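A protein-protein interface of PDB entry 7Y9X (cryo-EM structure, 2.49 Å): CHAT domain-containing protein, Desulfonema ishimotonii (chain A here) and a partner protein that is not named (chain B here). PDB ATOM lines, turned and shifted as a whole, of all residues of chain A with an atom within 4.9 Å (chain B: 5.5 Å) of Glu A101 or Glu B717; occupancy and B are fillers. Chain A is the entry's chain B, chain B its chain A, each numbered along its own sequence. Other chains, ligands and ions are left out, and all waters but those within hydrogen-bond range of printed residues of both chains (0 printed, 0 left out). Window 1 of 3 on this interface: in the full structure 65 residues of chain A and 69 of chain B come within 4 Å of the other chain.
Glu A101 touches just these residues of chain B: Ser B704 (3.1 Å) and Glu B717 (3.7 Å). Of chain A, only Glu A101 (3.7 Å) comes within 4 Å of Glu B717. Of the printed residues of chain A, Tyr B718 touches Arg A97 (3.9 Å). Of the printed residues of chain B, Glu A98 touches Ser B704. Of the printed residues of chain B, Arg A97 touches Tyr B718. Of the printed residues of chain A, Leu B377 touches Ile A104 (3.8 Å). Of the printed residues of chain A, Ile B376 touches Ile A104 and Arg A105. Leu A100 touches none of the printed residues of chain B. The nearest residue of chain B that does not touch Glu A101 is Leu B377 (4.7 Å). The nearest printed residue of chain A that does not touch Glu B717 is Arg A105 (5.3 Å). The nearest printed residue of chain B that does not touch Arg A105 is Glu B717 (5.3 Å).
The side-chain carboxylate of Glu A101 lies within hydrogen-bond range of the side-chain hydroxyl of Ser B704 (3.1 Å). The backbone carbonyl oxygen (O) of Ser B704 lies close to the side-chain carboxylate (OE2) of Glu A98, 2.9 Å away.
Printed residues of chain B that touch a printed residue of chain A: Ile B376, Leu B377, Ser B704, Glu B717 and Tyr B718. Hydrophobic or aromatic side chains of chain B within 4 Å of the printed part of chain A: Ile B376, Leu B377 and Tyr B718. Of the 9 printed residues of chain A, 5 touch a printed residue of chain B.
Tyr B718 touches Arg A97. Glu A101 touches Glu B717. Ile B376 touches Ile A104 (CD1 to O, 3.4 Å). CD1 of Ile A104 touches CD2 of Leu B377, 3.8 Å away. Arg A105 touches Ile B376 (CA to CD1, 3.6 Å).
NH2 of Arg A105 lies within salt-bridge range of OE2 of Glu A101. The side-chain amide oxygen of Gln A102 sits at hydrogen-bond distance from the guanidinium group of Arg A105 (3.2 Å). NZ of Lys B182 sits at hydrogen-bond distance from O of Glu B717 (2.6 Å). The side-chain hydroxyl of Ser B704 sits at hydrogen-bond distance from the side-chain carboxylate of Glu B717 (3.3 Å). The backbone NH (N) of Tyr B718 lies close to the side-chain hydroxyl (OG) of Ser B716 (3.4 Å).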
ATOM      1  N   ARG A  97      15.036  -6.117  34.828  1.00  0.00           N
ATOM      2  CA  ARG A  97      14.709  -4.739  34.477  1.00  0.00           C
ATOM      3  C   ARG A  97      15.188  -4.393  33.071  1.00  0.00           C
ATOM      4  O   ARG A  97      14.506  -3.669  32.337  1.00  0.00           O
ATOM      5  CB  ARG A  97      15.308  -3.782  35.507  1.00  0.00           C
ATOM      6  CG  ARG A  97      14.977  -2.323  35.270  1.00  0.00           C
ATOM      7  CD  ARG A  97      15.565  -1.412  36.337  1.00  0.00           C
ATOM      8  NE  ARG A  97      15.000  -1.649  37.660  1.00  0.00           N
ATOM      9  CZ  ARG A  97      15.605  -2.324  38.626  1.00  0.00           C
ATOM     10  NH1 ARG A  97      16.810  -2.841  38.458  1.00  0.00           N
ATOM     11  NH2 ARG A  97      14.990  -2.476  39.794  1.00  0.00           N
ATOM     12  N   GLU A  98      16.365  -4.889  32.683  1.00  0.00           N
ATOM     13  CA  GLU A  98      16.878  -4.617  31.343  1.00  0.00           C
ATOM     14  C   GLU A  98      16.032  -5.291  30.271  1.00  0.00           C
ATOM     15  O   GLU A  98      15.724  -4.681  29.243  1.00  0.00           O
ATOM     16  CB  GLU A  98      18.328  -5.082  31.221  1.00  0.00           C
ATOM     17  CG  GLU A  98      19.310  -4.354  32.111  1.00  0.00           C
ATOM     18  CD  GLU A  98      20.715  -4.897  31.964  1.00  0.00           C
ATOM     19  OE1 GLU A  98      20.934  -5.729  31.059  1.00  0.00           O
ATOM     20  OE2 GLU A  98      21.596  -4.501  32.755  1.00  0.00           O
ATOM     21  N   THR A  99      15.665  -6.556  30.478  1.00  0.00           N
ATOM     22  CA  THR A  99      14.936  -7.279  29.444  1.00  0.00           C
ATOM     23  C   THR A  99      13.516  -6.752  29.302  1.00  0.00           C
ATOM     24  O   THR A  99      12.963  -6.736  28.199  1.00  0.00           O
ATOM     25  CB  THR A  99      14.933  -8.775  29.746  1.00  0.00           C
ATOM     26  OG1 THR A  99      16.231  -9.168  30.210  1.00  0.00           O
ATOM     27  CG2 THR A  99      14.608  -9.558  28.490  1.00  0.00           C
ATOM     28  N   LEU A 100      12.912  -6.313  30.408  1.00  0.00           N
ATOM     29  CA  LEU A 100      11.619  -5.642  30.326  1.00  0.00           C
ATOM     30  C   LEU A 100      11.720  -4.348  29.533  1.00  0.00           C
ATOM     31  O   LEU A 100      10.743  -3.926  28.906  1.00  0.00           O
ATOM     32  CB  LEU A 100      11.086  -5.366  31.730  1.00  0.00           C
ATOM     33  CG  LEU A 100      10.592  -6.572  32.524  1.00  0.00           C
ATOM     34  CD1 LEU A 100      10.314  -6.179  33.955  1.00  0.00           C
ATOM     35  CD2 LEU A 100       9.349  -7.149  31.882  1.00  0.00           C
ATOM     36  N   GLU A 101      12.884  -3.698  29.568  1.00  0.00           N
ATOM     37  CA  GLU A 101      13.101  -2.498  28.769  1.00  0.00           C
ATOM     38  C   GLU A 101      13.018  -2.802  27.280  1.00  0.00           C
ATOM     39  O   GLU A 101      12.426  -2.036  26.511  1.00  0.00           O
ATOM     40  CB  GLU A 101      14.458  -1.886  29.120  1.00  0.00           C
ATOM     41  CG  GLU A 101      14.913  -0.771  28.199  1.00  0.00           C
ATOM     42  CD  GLU A 101      16.343  -0.342  28.463  1.00  0.00           C
ATOM     43  OE1 GLU A 101      16.970  -0.889  29.391  1.00  0.00           O
ATOM     44  OE2 GLU A 101      16.841   0.543  27.738  1.00  0.00           O
ATOM     45  N   GLN A 102      13.605  -3.922  26.855  1.00  0.00           N
ATOM     46  CA  GLN A 102      13.622  -4.260  25.437  1.00  0.00           C
ATOM     47  C   GLN A 102      12.248  -4.697  24.952  1.00  0.00           C
ATOM     48  O   GLN A 102      11.843  -4.361  23.835  1.00  0.00           O
ATOM     49  CB  GLN A 102      14.658  -5.349  25.177  1.00  0.00           C
ATOM     50  CG  GLN A 102      16.031  -4.994  25.698  1.00  0.00           C
ATOM     51  CD  GLN A 102      16.553  -3.703  25.105  1.00  0.00           C
ATOM     52  OE1 GLN A 102      17.086  -2.853  25.816  1.00  0.00           O
ATOM     53  NE2 GLN A 102      16.413  -3.552  23.794  1.00  0.00           N
ATOM     54  N   ILE A 103      11.517  -5.447  25.773  1.00  0.00           N
ATOM     55  CA  ILE A 103      10.194  -5.905  25.367  1.00  0.00           C
ATOM     56  C   ILE A 103       9.251  -4.724  25.179  1.00  0.00           C
ATOM     57  O   ILE A 103       8.486  -4.675  24.211  1.00  0.00           O
ATOM     58  CB  ILE A 103       9.651  -6.919  26.388  1.00  0.00           C
ATOM     59  CG1 ILE A 103      10.597  -8.111  26.488  1.00  0.00           C
ATOM     60  CG2 ILE A 103       8.272  -7.394  25.988  1.00  0.00           C
ATOM     61  CD1 ILE A 103      10.127  -9.167  27.429  1.00  0.00           C
ATOM     62  N   ILE A 104       9.299  -3.744  26.082  1.00  0.00           N
ATOM     63  CA  ILE A 104       8.374  -2.617  25.994  1.00  0.00           C
ATOM     64  C   ILE A 104       8.596  -1.834  24.706  1.00  0.00           C
ATOM     65  O   ILE A 104       7.638  -1.451  24.023  1.00  0.00           O
ATOM     66  CB  ILE A 104       8.507  -1.716  27.235  1.00  0.00           C
ATOM     67  CG1 ILE A 104       7.920  -2.407  28.466  1.00  0.00           C
ATOM     68  CG2 ILE A 104       7.818  -0.390  27.005  1.00  0.00           C
ATOM     69  CD1 ILE A 104       7.953  -1.555  29.711  1.00  0.00           C
ATOM     70  N   ARG A 105       9.856  -1.592  24.346  1.00  0.00           N
ATOM     71  CA  ARG A 105      10.152  -0.747  23.194  1.00  0.00           C
ATOM     72  C   ARG A 105       9.848  -1.452  21.877  1.00  0.00           C
ATOM     73  O   ARG A 105       9.482  -0.802  20.893  1.00  0.00           O
ATOM     74  CB  ARG A 105      11.609  -0.293  23.252  1.00  0.00           C
ATOM     75  CG  ARG A 105      12.621  -1.420  23.178  1.00  0.00           C
ATOM     76  CD  ARG A 105      14.027  -0.890  23.322  1.00  0.00           C
ATOM     77  NE  ARG A 105      14.070   0.141  24.348  1.00  0.00           N
ATOM     78  CZ  ARG A 105      15.176   0.572  24.938  1.00  0.00           C
ATOM     79  NH1 ARG A 105      16.359   0.055  24.649  1.00  0.00           N
ATOM     80  NH2 ARG A 105      15.092   1.540  25.846  1.00  0.00           N
ATOM     81  N   LYS B 182      19.935  13.822  36.377  1.00  0.00           N
ATOM     82  CA  LYS B 182      18.917  13.353  35.455  1.00  0.00           C
ATOM     83  C   LYS B 182      17.544  13.681  36.012  1.00  0.00           C
ATOM     84  O   LYS B 182      17.325  13.612  37.223  1.00  0.00           O
ATOM     85  CB  LYS B 182      19.044  11.845  35.229  1.00  0.00           C
ATOM     86  CG  LYS B 182      17.928  11.243  34.417  1.00  0.00           C
ATOM     87  CD  LYS B 182      17.973   9.742  34.453  1.00  0.00           C
ATOM     88  CE  LYS B 182      16.833   9.150  33.659  1.00  0.00           C
ATOM     89  NZ  LYS B 182      16.854   7.671  33.727  1.00  0.00           N
ATOM     90  N   ILE B 376      10.803   5.884  24.612  1.00  0.00           N
ATOM     91  CA  ILE B 376       9.768   5.137  25.313  1.00  0.00           C
ATOM     92  C   ILE B 376      10.102   5.116  26.798  1.00  0.00           C
ATOM     93  O   ILE B 376      11.242   5.353  27.205  1.00  0.00           O
ATOM     94  CB  ILE B 376       9.618   3.701  24.765  1.00  0.00           C
ATOM     95  CG1 ILE B 376       8.197   3.193  24.988  1.00  0.00           C
ATOM     96  CG2 ILE B 376      10.628   2.764  25.412  1.00  0.00           C
ATOM     97  CD1 ILE B 376       7.929   1.893  24.315  1.00  0.00           C
ATOM     98  N   LEU B 377       9.082   4.822  27.611  1.00  0.00           N
ATOM     99  CA  LEU B 377       9.192   4.870  29.071  1.00  0.00           C
ATOM    100  C   LEU B 377       9.657   6.248  29.541  1.00  0.00           C
ATOM    101  O   LEU B 377      10.452   6.373  30.474  1.00  0.00           O
ATOM    102  CB  LEU B 377      10.123   3.774  29.598  1.00  0.00           C
ATOM    103  CG  LEU B 377       9.643   2.323  29.539  1.00  0.00           C
ATOM    104  CD1 LEU B 377      10.763   1.382  29.928  1.00  0.00           C
ATOM    105  CD2 LEU B 377       8.456   2.123  30.456  1.00  0.00           C
ATOM    106  N   ARG B 503      25.483   5.298  16.543  1.00  0.00           N
ATOM    107  CA  ARG B 503      26.127   4.426  17.509  1.00  0.00           C
ATOM    108  C   ARG B 503      26.901   3.376  16.731  1.00  0.00           C
ATOM    109  O   ARG B 503      26.414   2.869  15.716  1.00  0.00           O
ATOM    110  CB  ARG B 503      25.115   3.771  18.454  1.00  0.00           C
ATOM    111  CG  ARG B 503      25.740   2.801  19.444  1.00  0.00           C
ATOM    112  CD  ARG B 503      24.720   2.224  20.407  1.00  0.00           C
ATOM    113  NE  ARG B 503      24.178   3.244  21.296  1.00  0.00           N
ATOM    114  CZ  ARG B 503      23.363   3.004  22.314  1.00  0.00           C
ATOM    115  NH1 ARG B 503      22.978   1.776  22.615  1.00  0.00           N
ATOM    116  NH2 ARG B 503      22.928   4.020  23.051  1.00  0.00           N
ATOM    117  N   HIS B 703      25.501  -1.440  29.505  1.00  0.00           N
ATOM    118  CA  HIS B 703      25.657  -0.135  30.147  1.00  0.00           C
ATOM    119  C   HIS B 703      24.314   0.538  30.399  1.00  0.00           C
ATOM    120  O   HIS B 703      24.223   1.765  30.467  1.00  0.00           O
ATOM    121  CB  HIS B 703      26.577   0.778  29.335  1.00  0.00           C
ATOM    122  CG  HIS B 703      27.986   0.289  29.268  1.00  0.00           C
ATOM    123  ND1 HIS B 703      28.792   0.192  30.380  1.00  0.00           N
ATOM    124  CD2 HIS B 703      28.730  -0.137  28.223  1.00  0.00           C
ATOM    125  CE1 HIS B 703      29.975  -0.272  30.021  1.00  0.00           C
ATOM    126  NE2 HIS B 703      29.962  -0.483  28.720  1.00  0.00           N
ATOM    127  N   SER B 704      23.266  -0.265  30.526  1.00  0.00           N
ATOM    128  CA  SER B 704      21.964   0.191  30.981  1.00  0.00           C
ATOM    129  C   SER B 704      21.720  -0.420  32.351  1.00  0.00           C
ATOM    130  O   SER B 704      21.858  -1.636  32.521  1.00  0.00           O
ATOM    131  CB  SER B 704      20.861  -0.211  30.000  1.00  0.00           C
ATOM    132  OG  SER B 704      19.602   0.277  30.427  1.00  0.00           O
ATOM    133  N   GLY B 715      28.964   8.720  32.170  1.00  0.00           N
ATOM    134  CA  GLY B 715      27.542   8.749  32.416  1.00  0.00           C
ATOM    135  C   GLY B 715      26.821   7.560  31.825  1.00  0.00           C
ATOM    136  O   GLY B 715      27.390   6.705  31.146  1.00  0.00           O
ATOM    137  N   SER B 716      25.524   7.509  32.101  1.00  0.00           N
ATOM    138  CA  SER B 716      24.670   6.434  31.622  1.00  0.00           C
ATOM    139  C   SER B 716      23.251   6.969  31.511  1.00  0.00           C
ATOM    140  O   SER B 716      23.011   8.173  31.623  1.00  0.00           O
ATOM    141  CB  SER B 716      24.756   5.212  32.544  1.00  0.00           C
ATOM    142  OG  SER B 716      24.262   5.504  33.838  1.00  0.00           O
ATOM    143  N   GLU B 717      22.303   6.062  31.292  1.00  0.00           N
ATOM    144  CA  GLU B 717      20.899   6.434  31.207  1.00  0.00           C
ATOM    145  C   GLU B 717      20.314   6.820  32.557  1.00  0.00           C
ATOM    146  O   GLU B 717      19.190   7.327  32.601  1.00  0.00           O
ATOM    147  CB  GLU B 717      20.102   5.283  30.599  1.00  0.00           C
ATOM    148  CG  GLU B 717      20.594   4.868  29.225  1.00  0.00           C
ATOM    149  CD  GLU B 717      19.823   3.698  28.646  1.00  0.00           C
ATOM    150  OE1 GLU B 717      18.807   3.292  29.249  1.00  0.00           O
ATOM    151  OE2 GLU B 717      20.243   3.175  27.592  1.00  0.00           O
ATOM    152  N   TYR B 718      21.044   6.599  33.649  1.00  0.00           N
ATOM    153  CA  TYR B 718      20.576   6.939  34.984  1.00  0.00           C
ATOM    154  C   TYR B 718      21.370   8.048  35.654  1.00  0.00           C
ATOM    155  O   TYR B 718      20.800   8.799  36.444  1.00  0.00           O
ATOM    156  CB  TYR B 718      20.601   5.700  35.885  1.00  0.00           C
ATOM    157  CG  TYR B 718      19.608   4.639  35.478  1.00  0.00           C
ATOM    158  CD1 TYR B 718      18.315   4.643  35.974  1.00  0.00           C
ATOM    159  CD2 TYR B 718      19.966   3.630  34.596  1.00  0.00           C
ATOM    160  CE1 TYR B 718      17.405   3.676  35.601  1.00  0.00           C
ATOM    161  CE2 TYR B 718      19.065   2.663  34.217  1.00  0.00           C
ATOM    162  CZ  TYR B 718      17.788   2.685  34.723  1.00  0.00           C
ATOM    163  OH  TYR B 718      16.891   1.713  34.344  1.00  0.00           O
ATOM    164  N   GLU B 719      22.661   8.167  35.366  1.00  0.00           N
ATOM    165  CA  GLU B 719      23.517   9.181  35.965  1.00  0.00           C
ATOM    166  C   GLU B 719      24.216   9.985  34.878  1.00  0.00           C
ATOM    167  O   GLU B 719      24.768   9.419  33.931  1.00  0.00           O
ATOM    168  CB  GLU B 719      24.548   8.541  36.903  1.00  0.00           C
ATOM    169  CG  GLU B 719      25.327   7.392  36.278  1.00  0.00           C
ATOM    170  CD  GLU B 719      26.223   6.674  37.270  1.00  0.00           C
ATOM    171  OE1 GLU B 719      26.361   7.160  38.413  1.00  0.00           O
ATOM    172  OE2 GLU B 719      26.782   5.615  36.911  1.00  0.00           O
